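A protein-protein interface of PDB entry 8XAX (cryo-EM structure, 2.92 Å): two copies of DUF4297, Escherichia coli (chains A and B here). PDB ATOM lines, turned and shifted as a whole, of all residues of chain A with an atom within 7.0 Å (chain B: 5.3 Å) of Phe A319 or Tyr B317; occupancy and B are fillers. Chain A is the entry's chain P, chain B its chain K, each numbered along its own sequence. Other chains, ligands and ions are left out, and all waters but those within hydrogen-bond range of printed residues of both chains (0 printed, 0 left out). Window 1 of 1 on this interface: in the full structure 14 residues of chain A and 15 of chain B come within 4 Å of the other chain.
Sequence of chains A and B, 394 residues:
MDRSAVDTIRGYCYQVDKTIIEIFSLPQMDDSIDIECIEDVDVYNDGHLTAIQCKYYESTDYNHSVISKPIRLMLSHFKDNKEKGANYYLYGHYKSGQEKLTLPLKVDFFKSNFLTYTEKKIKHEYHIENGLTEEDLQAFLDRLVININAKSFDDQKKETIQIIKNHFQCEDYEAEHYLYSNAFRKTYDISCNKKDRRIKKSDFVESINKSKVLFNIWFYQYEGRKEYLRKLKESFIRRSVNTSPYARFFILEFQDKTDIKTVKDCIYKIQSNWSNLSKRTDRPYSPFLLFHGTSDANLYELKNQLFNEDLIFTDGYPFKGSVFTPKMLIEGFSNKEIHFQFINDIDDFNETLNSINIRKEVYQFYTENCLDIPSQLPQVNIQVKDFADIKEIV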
ATOM      1  N   GLY A 316     -14.330  10.242  20.821  1.00  0.00           N
ATOM      2  CA  GLY A 316     -14.902  10.407  22.138  1.00  0.00           C
ATOM      3  C   GLY A 316     -15.278  11.822  22.499  1.00  0.00           C
ATOM      4  O   GLY A 316     -15.634  12.077  23.655  1.00  0.00           O
ATOM      5  N   TYR A 317     -15.215  12.754  21.549  1.00  0.00           N
ATOM      6  CA  TYR A 317     -15.600  14.147  21.768  1.00  0.00           C
ATOM      7  C   TYR A 317     -16.628  14.524  20.712  1.00  0.00           C
ATOM      8  O   TYR A 317     -16.297  15.149  19.695  1.00  0.00           O
ATOM      9  CB  TYR A 317     -14.385  15.075  21.729  1.00  0.00           C
ATOM     10  CG  TYR A 317     -13.329  14.733  22.755  1.00  0.00           C
ATOM     11  CD1 TYR A 317     -13.445  15.169  24.069  1.00  0.00           C
ATOM     12  CD2 TYR A 317     -12.218  13.975  22.411  1.00  0.00           C
ATOM     13  CE1 TYR A 317     -12.483  14.858  25.013  1.00  0.00           C
ATOM     14  CE2 TYR A 317     -11.252  13.660  23.348  1.00  0.00           C
ATOM     15  CZ  TYR A 317     -11.389  14.104  24.645  1.00  0.00           C
ATOM     16  OH  TYR A 317     -10.428  13.791  25.577  1.00  0.00           O
ATOM     17  N   PRO A 318     -17.894  14.150  20.919  1.00  0.00           N
ATOM     18  CA  PRO A 318     -18.922  14.442  19.909  1.00  0.00           C
ATOM     19  C   PRO A 318     -19.294  15.911  19.820  1.00  0.00           C
ATOM     20  O   PRO A 318     -19.838  16.329  18.790  1.00  0.00           O
ATOM     21  CB  PRO A 318     -20.112  13.594  20.369  1.00  0.00           C
ATOM     22  CG  PRO A 318     -19.934  13.498  21.844  1.00  0.00           C
ATOM     23  CD  PRO A 318     -18.455  13.468  22.099  1.00  0.00           C
ATOM     24  N   PHE A 319     -19.029  16.704  20.855  1.00  0.00           N
ATOM     25  CA  PHE A 319     -19.345  18.124  20.837  1.00  0.00           C
ATOM     26  C   PHE A 319     -18.243  18.895  21.549  1.00  0.00           C
ATOM     27  O   PHE A 319     -17.400  18.321  22.242  1.00  0.00           O
ATOM     28  CB  PHE A 319     -20.724  18.411  21.460  1.00  0.00           C
ATOM     29  CG  PHE A 319     -20.915  17.855  22.843  1.00  0.00           C
ATOM     30  CD1 PHE A 319     -20.631  18.624  23.961  1.00  0.00           C
ATOM     31  CD2 PHE A 319     -21.412  16.575  23.027  1.00  0.00           C
ATOM     32  CE1 PHE A 319     -20.821  18.118  25.232  1.00  0.00           C
ATOM     33  CE2 PHE A 319     -21.600  16.063  24.296  1.00  0.00           C
ATOM     34  CZ  PHE A 319     -21.305  16.836  25.400  1.00  0.00           C
ATOM     35  N   LYS A 320     -18.243  20.211  21.348  1.00  0.00           N
ATOM     36  CA  LYS A 320     -17.242  21.065  21.968  1.00  0.00           C
ATOM     37  C   LYS A 320     -17.475  21.157  23.471  1.00  0.00           C
ATOM     38  O   LYS A 320     -18.611  21.305  23.932  1.00  0.00           O
ATOM     39  CB  LYS A 320     -17.266  22.460  21.343  1.00  0.00           C
ATOM     40  CG  LYS A 320     -16.099  23.344  21.756  1.00  0.00           C
ATOM     41  CD  LYS A 320     -15.367  23.907  20.551  1.00  0.00           C
ATOM     42  CE  LYS A 320     -15.919  25.265  20.154  1.00  0.00           C
ATOM     43  NZ  LYS A 320     -15.517  26.328  21.115  1.00  0.00           N
ATOM     44  N   GLY A 321     -16.390  21.069  24.235  1.00  0.00           N
ATOM     45  CA  GLY A 321     -16.480  21.087  25.678  1.00  0.00           C
ATOM     46  C   GLY A 321     -16.912  19.783  26.306  1.00  0.00           C
ATOM     47  O   GLY A 321     -17.222  19.761  27.503  1.00  0.00           O
ATOM     48  N   SER A 322     -16.944  18.698  25.540  1.00  0.00           N
ATOM     49  CA  SER A 322     -17.373  17.410  26.058  1.00  0.00           C
ATOM     50  C   SER A 322     -16.280  16.760  26.893  1.00  0.00           C
ATOM     51  O   SER A 322     -15.086  16.993  26.689  1.00  0.00           O
ATOM     52  CB  SER A 322     -17.752  16.468  24.916  1.00  0.00           C
ATOM     53  OG  SER A 322     -16.604  15.829  24.396  1.00  0.00           O
ATOM     54  N   VAL A 323     -16.708  15.934  27.843  1.00  0.00           N
ATOM     55  CA  VAL A 323     -15.793  15.001  28.480  1.00  0.00           C
ATOM     56  C   VAL A 323     -15.524  13.840  27.530  1.00  0.00           C
ATOM     57  O   VAL A 323     -16.231  13.635  26.540  1.00  0.00           O
ATOM     58  CB  VAL A 323     -16.350  14.508  29.827  1.00  0.00           C
ATOM     59  CG1 VAL A 323     -16.675  15.688  30.728  1.00  0.00           C
ATOM     60  CG2 VAL A 323     -17.584  13.647  29.607  1.00  0.00           C
ATOM     61  N   THR A 325     -15.859  10.524  26.057  1.00  0.00           N
ATOM     62  CA  THR A 325     -16.901   9.504  26.071  1.00  0.00           C
ATOM     63  C   THR A 325     -16.430   8.292  25.283  1.00  0.00           C
ATOM     64  O   THR A 325     -16.485   8.298  24.043  1.00  0.00           O
ATOM     65  CB  THR A 325     -18.205  10.051  25.482  1.00  0.00           C
ATOM     66  OG1 THR A 325     -18.344  11.436  25.821  1.00  0.00           O
ATOM     67  CG2 THR A 325     -19.398   9.279  26.021  1.00  0.00           C
ATOM     68  N   TYR B 300     -21.325  24.141  28.530  1.00  0.00           N
ATOM     69  CA  TYR B 300     -20.795  22.796  28.332  1.00  0.00           C
ATOM     70  C   TYR B 300     -21.412  21.802  29.308  1.00  0.00           C
ATOM     71  O   TYR B 300     -21.553  20.619  28.977  1.00  0.00           O
ATOM     72  CB  TYR B 300     -19.272  22.800  28.472  1.00  0.00           C
ATOM     73  CG  TYR B 300     -18.547  23.544  27.371  1.00  0.00           C
ATOM     74  CD1 TYR B 300     -19.148  23.760  26.137  1.00  0.00           C
ATOM     75  CD2 TYR B 300     -17.262  24.035  27.571  1.00  0.00           C
ATOM     76  CE1 TYR B 300     -18.488  24.442  25.130  1.00  0.00           C
ATOM     77  CE2 TYR B 300     -16.595  24.717  26.569  1.00  0.00           C
ATOM     78  CZ  TYR B 300     -17.213  24.916  25.352  1.00  0.00           C
ATOM     79  OH  TYR B 300     -16.552  25.594  24.354  1.00  0.00           O
ATOM     80  N   LYS B 303     -24.708  20.882  27.840  1.00  0.00           N
ATOM     81  CA  LYS B 303     -24.477  19.981  26.716  1.00  0.00           C
ATOM     82  C   LYS B 303     -24.186  18.560  27.187  1.00  0.00           C
ATOM     83  O   LYS B 303     -24.645  17.589  26.574  1.00  0.00           O
ATOM     84  CB  LYS B 303     -23.318  20.498  25.866  1.00  0.00           C
ATOM     85  CG  LYS B 303     -23.699  21.364  24.683  1.00  0.00           C
ATOM     86  CD  LYS B 303     -22.500  22.184  24.230  1.00  0.00           C
ATOM     87  CE  LYS B 303     -22.336  22.154  22.720  1.00  0.00           C
ATOM     88  NZ  LYS B 303     -20.971  22.574  22.302  1.00  0.00           N
ATOM     89  N   ASN B 304     -23.418  18.420  28.270  1.00  0.00           N
ATOM     90  CA  ASN B 304     -23.056  17.094  28.759  1.00  0.00           C
ATOM     91  C   ASN B 304     -24.248  16.380  29.386  1.00  0.00           C
ATOM     92  O   ASN B 304     -24.393  15.161  29.237  1.00  0.00           O
ATOM     93  CB  ASN B 304     -21.908  17.202  29.762  1.00  0.00           C
ATOM     94  CG  ASN B 304     -20.562  17.367  29.089  1.00  0.00           C
ATOM     95  OD1 ASN B 304     -20.089  16.469  28.394  1.00  0.00           O
ATOM     96  ND2 ASN B 304     -19.936  18.521  29.292  1.00  0.00           N
ATOM     97  N   PHE B 307     -26.479  15.038  26.691  1.00  0.00           N
ATOM     98  CA  PHE B 307     -25.891  13.922  25.963  1.00  0.00           C
ATOM     99  C   PHE B 307     -25.939  12.629  26.765  1.00  0.00           C
ATOM    100  O   PHE B 307     -26.024  11.542  26.181  1.00  0.00           O
ATOM    101  CB  PHE B 307     -24.449  14.259  25.586  1.00  0.00           C
ATOM    102  CG  PHE B 307     -23.845  13.305  24.606  1.00  0.00           C
ATOM    103  CD1 PHE B 307     -24.086  13.450  23.251  1.00  0.00           C
ATOM    104  CD2 PHE B 307     -23.040  12.263  25.035  1.00  0.00           C
ATOM    105  CE1 PHE B 307     -23.534  12.580  22.341  1.00  0.00           C
ATOM    106  CE2 PHE B 307     -22.489  11.385  24.129  1.00  0.00           C
ATOM    107  CZ  PHE B 307     -22.741  11.545  22.781  1.00  0.00           C
ATOM    108  N   PHE B 313     -27.116  15.292  19.858  1.00  0.00           N
ATOM    109  CA  PHE B 313     -27.122  16.557  19.138  1.00  0.00           C
ATOM    110  C   PHE B 313     -25.806  16.740  18.394  1.00  0.00           C
ATOM    111  O   PHE B 313     -24.855  15.970  18.555  1.00  0.00           O
ATOM    112  CB  PHE B 313     -27.379  17.747  20.081  1.00  0.00           C
ATOM    113  CG  PHE B 313     -26.407  17.852  21.228  1.00  0.00           C
ATOM    114  CD1 PHE B 313     -25.256  18.617  21.114  1.00  0.00           C
ATOM    115  CD2 PHE B 313     -26.660  17.207  22.428  1.00  0.00           C
ATOM    116  CE1 PHE B 313     -24.368  18.721  22.165  1.00  0.00           C
ATOM    117  CE2 PHE B 313     -25.775  17.306  23.484  1.00  0.00           C
ATOM    118  CZ  PHE B 313     -24.629  18.065  23.352  1.00  0.00           C
ATOM    119  N   ASP B 315     -23.122  20.110  16.809  1.00  0.00           N
ATOM    120  CA  ASP B 315     -22.768  21.502  17.037  1.00  0.00           C
ATOM    121  C   ASP B 315     -21.869  22.091  15.961  1.00  0.00           C
ATOM    122  O   ASP B 315     -21.493  23.262  16.069  1.00  0.00           O
ATOM    123  CB  ASP B 315     -22.067  21.653  18.392  1.00  0.00           C
ATOM    124  CG  ASP B 315     -21.104  20.528  18.665  1.00  0.00           C
ATOM    125  OD1 ASP B 315     -21.495  19.357  18.480  1.00  0.00           O
ATOM    126  OD2 ASP B 315     -19.956  20.816  19.062  1.00  0.00           O
ATOM    127  N   GLY B 316     -21.515  21.325  14.934  1.00  0.00           N
ATOM    128  CA  GLY B 316     -20.521  21.757  13.980  1.00  0.00           C
ATOM    129  C   GLY B 316     -19.093  21.480  14.389  1.00  0.00           C
ATOM    130  O   GLY B 316     -18.171  21.841  13.646  1.00  0.00           O
ATOM    131  N   TYR B 317     -18.879  20.849  15.545  1.00  0.00           N
ATOM    132  CA  TYR B 317     -17.556  20.473  16.036  1.00  0.00           C
ATOM    133  C   TYR B 317     -17.587  18.971  16.294  1.00  0.00           C
ATOM    134  O   TYR B 317     -17.796  18.531  17.436  1.00  0.00           O
ATOM    135  CB  TYR B 317     -17.183  21.245  17.301  1.00  0.00           C
ATOM    136  CG  TYR B 317     -17.143  22.745  17.122  1.00  0.00           C
ATOM    137  CD1 TYR B 317     -15.994  23.380  16.672  1.00  0.00           C
ATOM    138  CD2 TYR B 317     -18.256  23.527  17.407  1.00  0.00           C
ATOM    139  CE1 TYR B 317     -15.953  24.752  16.509  1.00  0.00           C
ATOM    140  CE2 TYR B 317     -18.226  24.898  17.246  1.00  0.00           C
ATOM    141  CZ  TYR B 317     -17.073  25.506  16.797  1.00  0.00           C
ATOM    142  OH  TYR B 317     -17.038  26.871  16.637  1.00  0.00           O
ATOM    143  N   PRO B 318     -17.390  18.152  15.256  1.00  0.00           N
ATOM    144  CA  PRO B 318     -17.538  16.696  15.423  1.00  0.00           C
ATOM    145  C   PRO B 318     -16.420  16.040  16.216  1.00  0.00           C
ATOM    146  O   PRO B 318     -16.567  14.869  16.592  1.00  0.00           O
ATOM    147  CB  PRO B 318     -17.565  16.180  13.980  1.00  0.00           C
ATOM    148  CG  PRO B 318     -16.821  17.207  13.200  1.00  0.00           C
ATOM    149  CD  PRO B 318     -17.085  18.526  13.864  1.00  0.00           C
ATOM    150  N   PHE B 319     -15.320  16.738  16.486  1.00  0.00           N
ATOM    151  CA  PHE B 319     -14.223  16.160  17.249  1.00  0.00           C
ATOM    152  C   PHE B 319     -13.477  17.275  17.968  1.00  0.00           C
ATOM    153  O   PHE B 319     -13.702  18.462  17.723  1.00  0.00           O
ATOM    154  CB  PHE B 319     -13.283  15.336  16.355  1.00  0.00           C
ATOM    155  CG  PHE B 319     -12.779  16.067  15.138  1.00  0.00           C
ATOM    156  CD1 PHE B 319     -13.489  16.037  13.949  1.00  0.00           C
ATOM    157  CD2 PHE B 319     -11.576  16.753  15.176  1.00  0.00           C
ATOM    158  CE1 PHE B 319     -13.023  16.698  12.831  1.00  0.00           C
ATOM    159  CE2 PHE B 319     -11.100  17.411  14.058  1.00  0.00           C
ATOM    160  CZ  PHE B 319     -11.826  17.384  12.884  1.00  0.00           C
ATOM    161  N   SER B 322     -11.587  20.604  16.403  1.00  0.00           N
ATOM    162  CA  SER B 322     -12.128  20.849  15.076  1.00  0.00           C
ATOM    163  C   SER B 322     -12.481  22.317  14.888  1.00  0.00           C
ATOM    164  O   SER B 322     -12.858  23.019  15.831  1.00  0.00           O
ATOM    165  CB  SER B 322     -13.374  19.997  14.842  1.00  0.00           C
ATOM    166  OG  SER B 322     -14.089  20.443  13.702  1.00  0.00           O
ATOM    167  N   VAL B 323     -12.354  22.779  13.647  1.00  0.00           N
ATOM    168  CA  VAL B 323     -12.976  24.035  13.258  1.00  0.00           C
ATOM    169  C   VAL B 323     -14.479  23.819  13.111  1.00  0.00           C
ATOM    170  O   VAL B 323     -14.967  22.687  13.050  1.00  0.00           O
ATOM    171  CB  VAL B 323     -12.360  24.584  11.959  1.00  0.00           C
ATOM    172  CG1 VAL B 323     -11.009  25.222  12.241  1.00  0.00           C
ATOM    173  CG2 VAL B 323     -12.230  23.478  10.926  1.00  0.00           C
ATOM    174  N   PHE B 324     -15.223  24.921  13.065  1.00  0.00           N
ATOM    175  CA  PHE B 324     -16.672  24.824  12.951  1.00  0.00           C
ATOM    176  C   PHE B 324     -17.051  24.336  11.559  1.00  0.00           C
ATOM    177  O   PHE B 324     -16.672  24.943  10.553  1.00  0.00           O
ATOM    178  CB  PHE B 324     -17.329  26.170  13.238  1.00  0.00           C
ATOM    179  CG  PHE B 324     -18.812  26.176  13.007  1.00  0.00           C
ATOM    180  CD1 PHE B 324     -19.649  25.390  13.782  1.00  0.00           C
ATOM    181  CD2 PHE B 324     -19.370  26.963  12.013  1.00  0.00           C
ATOM    182  CE1 PHE B 324     -21.016  25.390  13.573  1.00  0.00           C
ATOM    183  CE2 PHE B 324     -20.737  26.968  11.798  1.00  0.00           C
ATOM    184  CZ  PHE B 324     -21.560  26.181  12.580  1.00  0.00           C
ATOM    185  N   THR B 325     -17.796  23.235  11.505  1.00  0.00           N
ATOM    186  CA  THR B 325     -18.258  22.672  10.241  1.00  0.00           C
ATOM    187  C   THR B 325     -19.758  22.900  10.135  1.00  0.00           C
ATOM    188  O   THR B 325     -20.541  22.160  10.749  1.00  0.00           O
ATOM    189  CB  THR B 325     -17.933  21.178  10.157  1.00  0.00           C
ATOM    190  OG1 THR B 325     -16.528  20.979  10.359  1.00  0.00           O
ATOM    191  CG2 THR B 325     -18.325  20.621   8.796  1.00  0.00           C
ATOM    192  N   ASN B 344     -23.322  27.170  18.963  1.00  0.00           N
ATOM    193  CA  ASN B 344     -22.531  27.571  20.122  1.00  0.00           C
ATOM    194  C   ASN B 344     -22.742  29.042  20.469  1.00  0.00           C
ATOM    195  O   ASN B 344     -23.200  29.372  21.568  1.00  0.00           O
ATOM    196  CB  ASN B 344     -21.051  27.280  19.871  1.00  0.00           C
ATOM    197  CG  ASN B 344     -20.564  26.054  20.618  1.00  0.00           C
ATOM    198  OD1 ASN B 344     -21.359  25.296  21.174  1.00  0.00           O
ATOM    199  ND2 ASN B 344     -19.253  25.854  20.635  1.00  0.00           N
ATOM    200  N   ASP B 348     -21.249  31.187  15.095  1.00  0.00           N
ATOM    201  CA  ASP B 348     -21.703  29.976  14.428  1.00  0.00           C
ATOM    202  C   ASP B 348     -23.118  30.098  13.876  1.00  0.00           C
ATOM    203  O   ASP B 348     -23.562  29.201  13.152  1.00  0.00           O
ATOM    204  CB  ASP B 348     -21.628  28.790  15.395  1.00  0.00           C
ATOM    205  CG  ASP B 348     -20.251  28.632  16.010  1.00  0.00           C
ATOM    206  OD1 ASP B 348     -19.326  28.183  15.305  1.00  0.00           O
ATOM    207  OD2 ASP B 348     -20.091  28.957  17.205  1.00  0.00           O
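The side-chain hydroxyl (OH) of Tyr B300 sits close to the side-chain amino group (NZ) of Lys A320 (3.5 Å). O of Lys A320 sits at hydrogen-bond distance from NZ of Lys B303, 3.1 Å away. The side-chain amide nitrogen (ND2) of Asn B304 lies within hydrogen-bond range of the backbone carbonyl oxygen (O) of Gly A321 (3.5 Å). N of Val A323 is in hydrogen-bond range of OD1 of Asn B304, 3.5 Å away. The side-chain carboxylate of Asp B315 lies within hydrogen-bond range of the backbone NH of Lys A320 (2.9 Å). The backbone carbonyl oxygen (O) of Tyr A317 lies close to the backbone carbonyl oxygen (O) of Pro B318, at 3.1 Å. O of Pro A318 lies close to OD1 of Asp B315 (3.5 Å). The backbone carbonyl oxygen (O) of Tyr B317 lies close to the backbone carbonyl oxygen (O) of Pro A318, 3.3 Å away.
Along chain B the printed residues that touch a printed residue of chain A span positions 300 to 344. Of the 9 printed residues of chain A, 7 touch a printed residue of chain B. Printed residues of chain A that touch a printed residue of chain B: Tyr A317, Pro A318, Phe A319, Lys A320, Gly A321, Ser A322 and Val A323. Hydrophobic or aromatic side chains of chain A that line the printed part of chain B: Pro A318, Phe A319 and Val A323. Among the printed residues, 20 pairs touch across the chains.
O of Tyr B300 is in hydrogen-bond range of ND2 of Asn B304. The side-chain amino group (NZ) of Lys B303 lies within salt-bridge range of the side-chain carboxylate (OD2) of Asp B315 (3.8 Å). The side-chain amino group (NZ) of Lys B303 sits at hydrogen-bond distance from the side-chain amide oxygen (OD1) of Asn B344. The side-chain carboxylate (OD1) of Asp B348 lies within hydrogen-bond range of the side-chain hydroxyl (OH) of Tyr B317, at 3.0 Å. The side-chain hydroxyl (OG) of Ser A322 sits close to the backbone carbonyl oxygen (O) of Phe A319 (3.4 Å). O of Val A323 is in hydrogen-bond range of OG1 of Thr A325, at 3.1 Å.
Of chain B, only Lys B303 (3.5 Å), Asn B304 (3.3 Å), Phe B307 (3.6 Å), Phe B313 (3.6 Å), Asp B315 (3.2 Å) and Tyr B317 (3.8 Å) come within 4 Å of Phe A319. Tyr B317 touches three residues of chain A. No residue of chain A comes within 4 Å of Gly B316. Of the printed residues of chain B, Tyr A317 touches Pro B318 (3.1 Å) and Phe B319 (3.4 Å). Of the printed residues of chain A, Pro B318 touches Tyr A317. Ser B322 touches none of the printed residues of chain A. The nearest residue of chain B that does not touch Phe A319 is Tyr B300 (4.6 Å). The nearest residue of chain A that does not touch Tyr B317 is Tyr A317 (4.3 Å).
Tyr A317 touches Pro B318, and with the chains exchanged Pro A318 touches Tyr B317. Tyr A317 touches Phe B319, and with the chains exchanged Phe A319 touches Tyr B317.
Among the printed residues, merely in contact across the chains: Phe A319 with Asp B315 (3.2 Å), Phe A319 with Asn B304 (3.3 Å), Tyr A317 with Phe B319 (3.4 Å), Lys A320 with Asn B344 (3.4 Å), Phe A319 with Lys B303 (3.5 Å), Pro A318 with Phe B307 (3.5 Å), Lys A320 with Tyr B317 (3.6 Å), Phe A319 with Phe B313 (3.6 Å), Phe A319 with Phe B307 (3.6 Å), Gly A321 with Tyr B300 (3.6 Å), Ser A322 with Asn B304 (3.7 Å) and Phe A319 with Tyr B317 (3.8 Å).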
